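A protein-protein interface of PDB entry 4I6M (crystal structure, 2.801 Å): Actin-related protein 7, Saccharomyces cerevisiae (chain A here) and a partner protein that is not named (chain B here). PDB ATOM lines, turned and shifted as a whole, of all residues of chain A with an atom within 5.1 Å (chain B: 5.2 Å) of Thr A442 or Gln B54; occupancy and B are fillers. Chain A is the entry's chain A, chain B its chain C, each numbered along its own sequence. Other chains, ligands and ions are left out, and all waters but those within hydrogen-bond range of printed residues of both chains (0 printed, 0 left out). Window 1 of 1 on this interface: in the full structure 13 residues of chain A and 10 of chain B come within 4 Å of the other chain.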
ATOM      1  N   ALA A 144     -33.185  26.727  18.136  1.00  0.00           N
ATOM      2  CA  ALA A 144     -32.379  26.391  19.299  1.00  0.00           C
ATOM      3  C   ALA A 144     -31.572  27.599  19.748  1.00  0.00           C
ATOM      4  O   ALA A 144     -31.595  27.959  20.922  1.00  0.00           O
ATOM      5  CB  ALA A 144     -31.468  25.225  18.983  1.00  0.00           C
ATOM      6  N   LEU A 147     -33.967  29.875  21.480  1.00  0.00           N
ATOM      7  CA  LEU A 147     -34.235  29.332  22.805  1.00  0.00           C
ATOM      8  C   LEU A 147     -33.041  29.491  23.754  1.00  0.00           C
ATOM      9  O   LEU A 147     -33.194  29.955  24.881  1.00  0.00           O
ATOM     10  CB  LEU A 147     -34.589  27.858  22.700  1.00  0.00           C
ATOM     11  CG  LEU A 147     -34.528  27.148  24.047  1.00  0.00           C
ATOM     12  CD1 LEU A 147     -35.823  27.375  24.813  1.00  0.00           C
ATOM     13  CD2 LEU A 147     -34.236  25.666  23.875  1.00  0.00           C
ATOM     14  N   SER A 148     -31.854  29.098  23.302  1.00  0.00           N
ATOM     15  CA  SER A 148     -30.639  29.240  24.103  1.00  0.00           C
ATOM     16  C   SER A 148     -30.467  30.679  24.595  1.00  0.00           C
ATOM     17  O   SER A 148     -29.665  30.952  25.477  1.00  0.00           O
ATOM     18  CB  SER A 148     -29.409  28.812  23.292  1.00  0.00           C
ATOM     19  OG  SER A 148     -28.780  29.915  22.643  1.00  0.00           O
ATOM     20  N   LEU A 438     -23.966  25.676  20.403  1.00  0.00           N
ATOM     21  CA  LEU A 438     -24.393  26.152  21.716  1.00  0.00           C
ATOM     22  C   LEU A 438     -25.888  26.008  21.914  1.00  0.00           C
ATOM     23  O   LEU A 438     -26.332  25.683  23.003  1.00  0.00           O
ATOM     24  CB  LEU A 438     -24.002  27.611  21.917  1.00  0.00           C
ATOM     25  CG  LEU A 438     -22.551  27.710  22.372  1.00  0.00           C
ATOM     26  CD1 LEU A 438     -22.179  29.127  22.738  1.00  0.00           C
ATOM     27  CD2 LEU A 438     -22.356  26.764  23.546  1.00  0.00           C
ATOM     28  N   GLY A 439     -26.659  26.264  20.861  1.00  0.00           N
ATOM     29  CA  GLY A 439     -28.099  26.111  20.907  1.00  0.00           C
ATOM     30  C   GLY A 439     -28.486  24.665  21.148  1.00  0.00           C
ATOM     31  O   GLY A 439     -29.216  24.355  22.093  1.00  0.00           O
ATOM     32  N   ALA A 440     -27.994  23.774  20.295  1.00  0.00           N
ATOM     33  CA  ALA A 440     -28.282  22.354  20.442  1.00  0.00           C
ATOM     34  C   ALA A 440     -27.908  21.888  21.852  1.00  0.00           C
ATOM     35  O   ALA A 440     -28.629  21.108  22.480  1.00  0.00           O
ATOM     36  CB  ALA A 440     -27.531  21.559  19.391  1.00  0.00           C
ATOM     37  N   LEU A 441     -26.783  22.386  22.355  1.00  0.00           N
ATOM     38  CA  LEU A 441     -26.334  22.058  23.702  1.00  0.00           C
ATOM     39  C   LEU A 441     -27.388  22.387  24.750  1.00  0.00           C
ATOM     40  O   LEU A 441     -27.621  21.587  25.655  1.00  0.00           O
ATOM     41  CB  LEU A 441     -25.035  22.795  24.047  1.00  0.00           C
ATOM     42  CG  LEU A 441     -24.443  22.497  25.425  1.00  0.00           C
ATOM     43  CD1 LEU A 441     -23.867  21.112  25.437  1.00  0.00           C
ATOM     44  CD2 LEU A 441     -23.365  23.472  25.771  1.00  0.00           C
ATOM     45  N   THR A 442     -28.026  23.555  24.639  1.00  0.00           N
ATOM     46  CA  THR A 442     -28.987  23.961  25.664  1.00  0.00           C
ATOM     47  C   THR A 442     -30.296  23.211  25.532  1.00  0.00           C
ATOM     48  O   THR A 442     -31.042  23.130  26.487  1.00  0.00           O
ATOM     49  CB  THR A 442     -29.238  25.478  25.732  1.00  0.00           C
ATOM     50  OG1 THR A 442     -30.460  25.790  25.079  1.00  0.00           O
ATOM     51  CG2 THR A 442     -28.110  26.259  25.094  1.00  0.00           C
ATOM     52  N   MET A 443     -30.560  22.651  24.354  1.00  0.00           N
ATOM     53  CA  MET A 443     -31.664  21.712  24.179  1.00  0.00           C
ATOM     54  C   MET A 443     -31.358  20.405  24.879  1.00  0.00           C
ATOM     55  O   MET A 443     -32.235  19.804  25.489  1.00  0.00           O
ATOM     56  CB  MET A 443     -31.870  21.372  22.710  1.00  0.00           C
ATOM     57  CG  MET A 443     -32.181  22.528  21.809  1.00  0.00           C
ATOM     58  SD  MET A 443     -33.940  23.191  22.129  1.00  0.00           S
ATOM     59  CE  MET A 443     -34.939  21.501  22.097  1.00  0.00           C
ATOM     60  N   ALA A 444     -30.116  19.941  24.749  1.00  0.00           N
ATOM     61  CA  ALA A 444     -29.720  18.655  25.316  1.00  0.00           C
ATOM     62  C   ALA A 444     -29.732  18.685  26.838  1.00  0.00           C
ATOM     63  O   ALA A 444     -29.831  17.654  27.484  1.00  0.00           O
ATOM     64  CB  ALA A 444     -28.356  18.245  24.807  1.00  0.00           C
ATOM     65  N   ASN A 445     -29.629  19.875  27.404  1.00  0.00           N
ATOM     66  CA  ASN A 445     -29.681  20.036  28.847  1.00  0.00           C
ATOM     67  C   ASN A 445     -31.067  20.437  29.346  1.00  0.00           C
ATOM     68  O   ASN A 445     -31.208  20.975  30.446  1.00  0.00           O
ATOM     69  CB  ASN A 445     -28.621  21.041  29.312  1.00  0.00           C
ATOM     70  CG  ASN A 445     -27.213  20.494  29.177  1.00  0.00           C
ATOM     71  OD1 ASN A 445     -26.768  19.664  29.977  1.00  0.00           O
ATOM     72  ND2 ASN A 445     -26.508  20.943  28.150  1.00  0.00           N
ATOM     73  N   LEU A 446     -32.093  20.188  28.537  1.00  0.00           N
ATOM     74  CA  LEU A 446     -33.453  20.469  28.981  1.00  0.00           C
ATOM     75  C   LEU A 446     -33.864  19.367  29.923  1.00  0.00           C
ATOM     76  O   LEU A 446     -33.511  18.206  29.735  1.00  0.00           O
ATOM     77  CB  LEU A 446     -34.439  20.597  27.822  1.00  0.00           C
ATOM     78  CG  LEU A 446     -34.371  21.907  27.047  1.00  0.00           C
ATOM     79  CD1 LEU A 446     -35.326  21.857  25.880  1.00  0.00           C
ATOM     80  CD2 LEU A 446     -34.676  23.076  27.953  1.00  0.00           C
ATOM     81  N   LYS B  49     -37.173  28.763  31.022  1.00  0.00           N
ATOM     82  CA  LYS B  49     -36.598  28.663  32.365  1.00  0.00           C
ATOM     83  C   LYS B  49     -35.265  27.924  32.340  1.00  0.00           C
ATOM     84  O   LYS B  49     -34.278  28.389  32.897  1.00  0.00           O
ATOM     85  CB  LYS B  49     -37.580  27.956  33.305  1.00  0.00           C
ATOM     86  CG  LYS B  49     -37.098  27.741  34.739  1.00  0.00           C
ATOM     87  CD  LYS B  49     -38.252  27.955  35.749  1.00  0.00           C
ATOM     88  CE  LYS B  49     -38.376  26.836  36.796  1.00  0.00           C
ATOM     89  NZ  LYS B  49     -37.290  26.879  37.821  1.00  0.00           N
ATOM     90  N   SER B  50     -35.232  26.775  31.681  1.00  0.00           N
ATOM     91  CA  SER B  50     -34.010  26.003  31.608  1.00  0.00           C
ATOM     92  C   SER B  50     -32.938  26.821  30.880  1.00  0.00           C
ATOM     93  O   SER B  50     -31.793  26.892  31.318  1.00  0.00           O
ATOM     94  CB  SER B  50     -34.260  24.681  30.885  1.00  0.00           C
ATOM     95  OG  SER B  50     -33.202  23.763  31.110  1.00  0.00           O
ATOM     96  N   ALA B  51     -33.319  27.448  29.772  1.00  0.00           N
ATOM     97  CA  ALA B  51     -32.374  28.233  28.998  1.00  0.00           C
ATOM     98  C   ALA B  51     -31.762  29.353  29.826  1.00  0.00           C
ATOM     99  O   ALA B  51     -30.546  29.573  29.798  1.00  0.00           O
ATOM    100  CB  ALA B  51     -33.031  28.786  27.759  1.00  0.00           C
ATOM    101  N   ILE B  52     -32.596  30.067  30.564  1.00  0.00           N
ATOM    102  CA  ILE B  52     -32.074  31.121  31.414  1.00  0.00           C
ATOM    103  C   ILE B  52     -31.196  30.564  32.527  1.00  0.00           C
ATOM    104  O   ILE B  52     -30.154  31.129  32.821  1.00  0.00           O
ATOM    105  CB  ILE B  52     -33.186  32.004  31.982  1.00  0.00           C
ATOM    106  CG1 ILE B  52     -33.859  32.760  30.839  1.00  0.00           C
ATOM    107  CG2 ILE B  52     -32.617  32.997  32.976  1.00  0.00           C
ATOM    108  CD1 ILE B  52     -35.310  33.083  31.131  1.00  0.00           C
ATOM    109  N   ASN B  53     -31.595  29.451  33.133  1.00  0.00           N
ATOM    110  CA  ASN B  53     -30.766  28.862  34.173  1.00  0.00           C
ATOM    111  C   ASN B  53     -29.411  28.388  33.666  1.00  0.00           C
ATOM    112  O   ASN B  53     -28.401  28.588  34.342  1.00  0.00           O
ATOM    113  CB  ASN B  53     -31.501  27.759  34.931  1.00  0.00           C
ATOM    114  CG  ASN B  53     -32.484  28.319  35.929  1.00  0.00           C
ATOM    115  OD1 ASN B  53     -32.304  29.434  36.428  1.00  0.00           O
ATOM    116  ND2 ASN B  53     -33.540  27.562  36.219  1.00  0.00           N
ATOM    117  N   GLN B  54     -29.386  27.787  32.477  1.00  0.00           N
ATOM    118  CA  GLN B  54     -28.140  27.307  31.873  1.00  0.00           C
ATOM    119  C   GLN B  54     -27.160  28.436  31.595  1.00  0.00           C
ATOM    120  O   GLN B  54     -25.972  28.307  31.890  1.00  0.00           O
ATOM    121  CB  GLN B  54     -28.407  26.503  30.600  1.00  0.00           C
ATOM    122  CG  GLN B  54     -29.222  25.245  30.847  1.00  0.00           C
ATOM    123  CD  GLN B  54     -29.416  24.427  29.592  1.00  0.00           C
ATOM    124  OE1 GLN B  54     -28.487  24.236  28.827  1.00  0.00           O
ATOM    125  NE2 GLN B  54     -30.626  23.943  29.376  1.00  0.00           N
ATOM    126  N   TYR B  55     -27.669  29.536  31.047  1.00  0.00           N
ATOM    127  CA  TYR B  55     -26.871  30.738  30.775  1.00  0.00           C
ATOM    128  C   TYR B  55     -26.239  31.328  32.038  1.00  0.00           C
ATOM    129  O   TYR B  55     -25.086  31.755  32.025  1.00  0.00           O
ATOM    130  CB  TYR B  55     -27.717  31.813  30.069  1.00  0.00           C
ATOM    131  CG  TYR B  55     -26.968  33.100  29.831  1.00  0.00           C
ATOM    132  CD1 TYR B  55     -26.229  33.287  28.661  1.00  0.00           C
ATOM    133  CD2 TYR B  55     -26.969  34.123  30.782  1.00  0.00           C
ATOM    134  CE1 TYR B  55     -25.518  34.453  28.431  1.00  0.00           C
ATOM    135  CE2 TYR B  55     -26.252  35.313  30.560  1.00  0.00           C
ATOM    136  CZ  TYR B  55     -25.529  35.466  29.377  1.00  0.00           C
ATOM    137  OH  TYR B  55     -24.811  36.621  29.125  1.00  0.00           O
ATOM    138  N   ASN B  56     -27.002  31.362  33.123  1.00  0.00           N
ATOM    139  CA  ASN B  56     -26.502  31.865  34.392  1.00  0.00           C
ATOM    140  C   ASN B  56     -25.466  30.921  34.988  1.00  0.00           C
ATOM    141  O   ASN B  56     -24.613  31.340  35.748  1.00  0.00           O
ATOM    142  CB  ASN B  56     -27.653  32.100  35.387  1.00  0.00           C
ATOM    143  CG  ASN B  56     -28.570  33.258  34.977  1.00  0.00           C
ATOM    144  OD1 ASN B  56     -28.201  34.112  34.162  1.00  0.00           O
ATOM    145  ND2 ASN B  56     -29.774  33.281  35.539  1.00  0.00           N
ATOM    146  N   ARG B  57     -25.545  29.642  34.636  1.00  0.00           N
ATOM    147  CA  ARG B  57     -24.611  28.636  35.128  1.00  0.00           C
ATOM    148  C   ARG B  57     -23.272  28.799  34.391  1.00  0.00           C
ATOM    149  O   ARG B  57     -22.200  28.788  35.012  1.00  0.00           O
ATOM    150  CB  ARG B  57     -25.204  27.243  34.935  1.00  0.00           C
ATOM    151  CG  ARG B  57     -24.374  26.079  35.443  1.00  0.00           C
ATOM    152  CD  ARG B  57     -25.201  24.794  35.393  1.00  0.00           C
ATOM    153  NE  ARG B  57     -26.546  24.987  35.946  1.00  0.00           N
ATOM    154  CZ  ARG B  57     -27.676  24.545  35.391  1.00  0.00           C
ATOM    155  NH1 ARG B  57     -27.656  23.867  34.249  1.00  0.00           N
ATOM    156  NH2 ARG B  57     -28.837  24.784  35.984  1.00  0.00           N
ATOM    157  N   ARG B  58     -23.329  29.001  33.075  1.00  0.00           N
ATOM    158  CA  ARG B  58     -22.125  29.376  32.349  1.00  0.00           C
ATOM    159  C   ARG B  58     -21.403  30.514  33.054  1.00  0.00           C
ATOM    160  O   ARG B  58     -20.232  30.400  33.403  1.00  0.00           O
ATOM    161  CB  ARG B  58     -22.454  29.863  30.951  1.00  0.00           C
ATOM    162  CG  ARG B  58     -22.712  28.776  29.960  1.00  0.00           C
ATOM    163  CD  ARG B  58     -22.393  29.237  28.533  1.00  0.00           C
ATOM    164  NE  ARG B  58     -22.237  28.057  27.697  1.00  0.00           N
ATOM    165  CZ  ARG B  58     -21.175  27.823  26.945  1.00  0.00           C
ATOM    166  NH1 ARG B  58     -20.187  28.702  26.895  1.00  0.00           N
ATOM    167  NH2 ARG B  58     -21.117  26.718  26.229  1.00  0.00           N
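The backbone carbonyl oxygen (O) of Thr A442 is in hydrogen-bond range of the side-chain amide nitrogen (NE2) of Gln B54, at 3.0 Å. The side-chain hydroxyl (OG) of Ser B50 sits at hydrogen-bond distance from the backbone carbonyl oxygen (O) of Asn A445 (3.5 Å). The side-chain amide nitrogen (NE2) of Gln B54 is in hydrogen-bond range of the backbone carbonyl oxygen (O) of Asn A445 (3.2 Å).
The backbone carbonyl oxygen of Leu A441 sits at hydrogen-bond distance from the side-chain amide nitrogen of Asn A445. OG of Ser B50 is in hydrogen-bond range of NE2 of Gln B54, 3.1 Å away.
Leu A147 touches Ala B51 (O to CB, 3.1 Å). Leu A438 touches Arg B58 (CD2 to NH2, 3.0 Å). Leu A441 touches Arg B58 (CD2 to NH2, 3.97 Å). Ser B50 touches Leu A446 (CB to CD2, 3.4 Å).
Printed residues of chain B within 4 Å of Thr A442: Gln B54 (3.0 Å). Of the printed residues of chain A, Gln B54 touches Thr A442 (3.0 Å) and Asn A445 (3.2 Å). Printed residues of chain A within 4 Å of Ala B51: Leu A147 (3.1 Å). Of the printed residues of chain A, Ser B50 touches Asn A445 and Leu A446. Of the printed residues of chain B, Leu A446 touches Ser B50 (3.4 Å). Printed residues of chain A within 4 Å of Arg B58: Leu A438 (3.0 Å) and Leu A441 (3.97 Å). Lys B49 touches none of the printed residues of chain A.
Hydrophobic or aromatic side chains of chain B within 4 Å of the printed part of chain A: Ala B51. Among the printed residues, 7 pairs touch across the chains.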
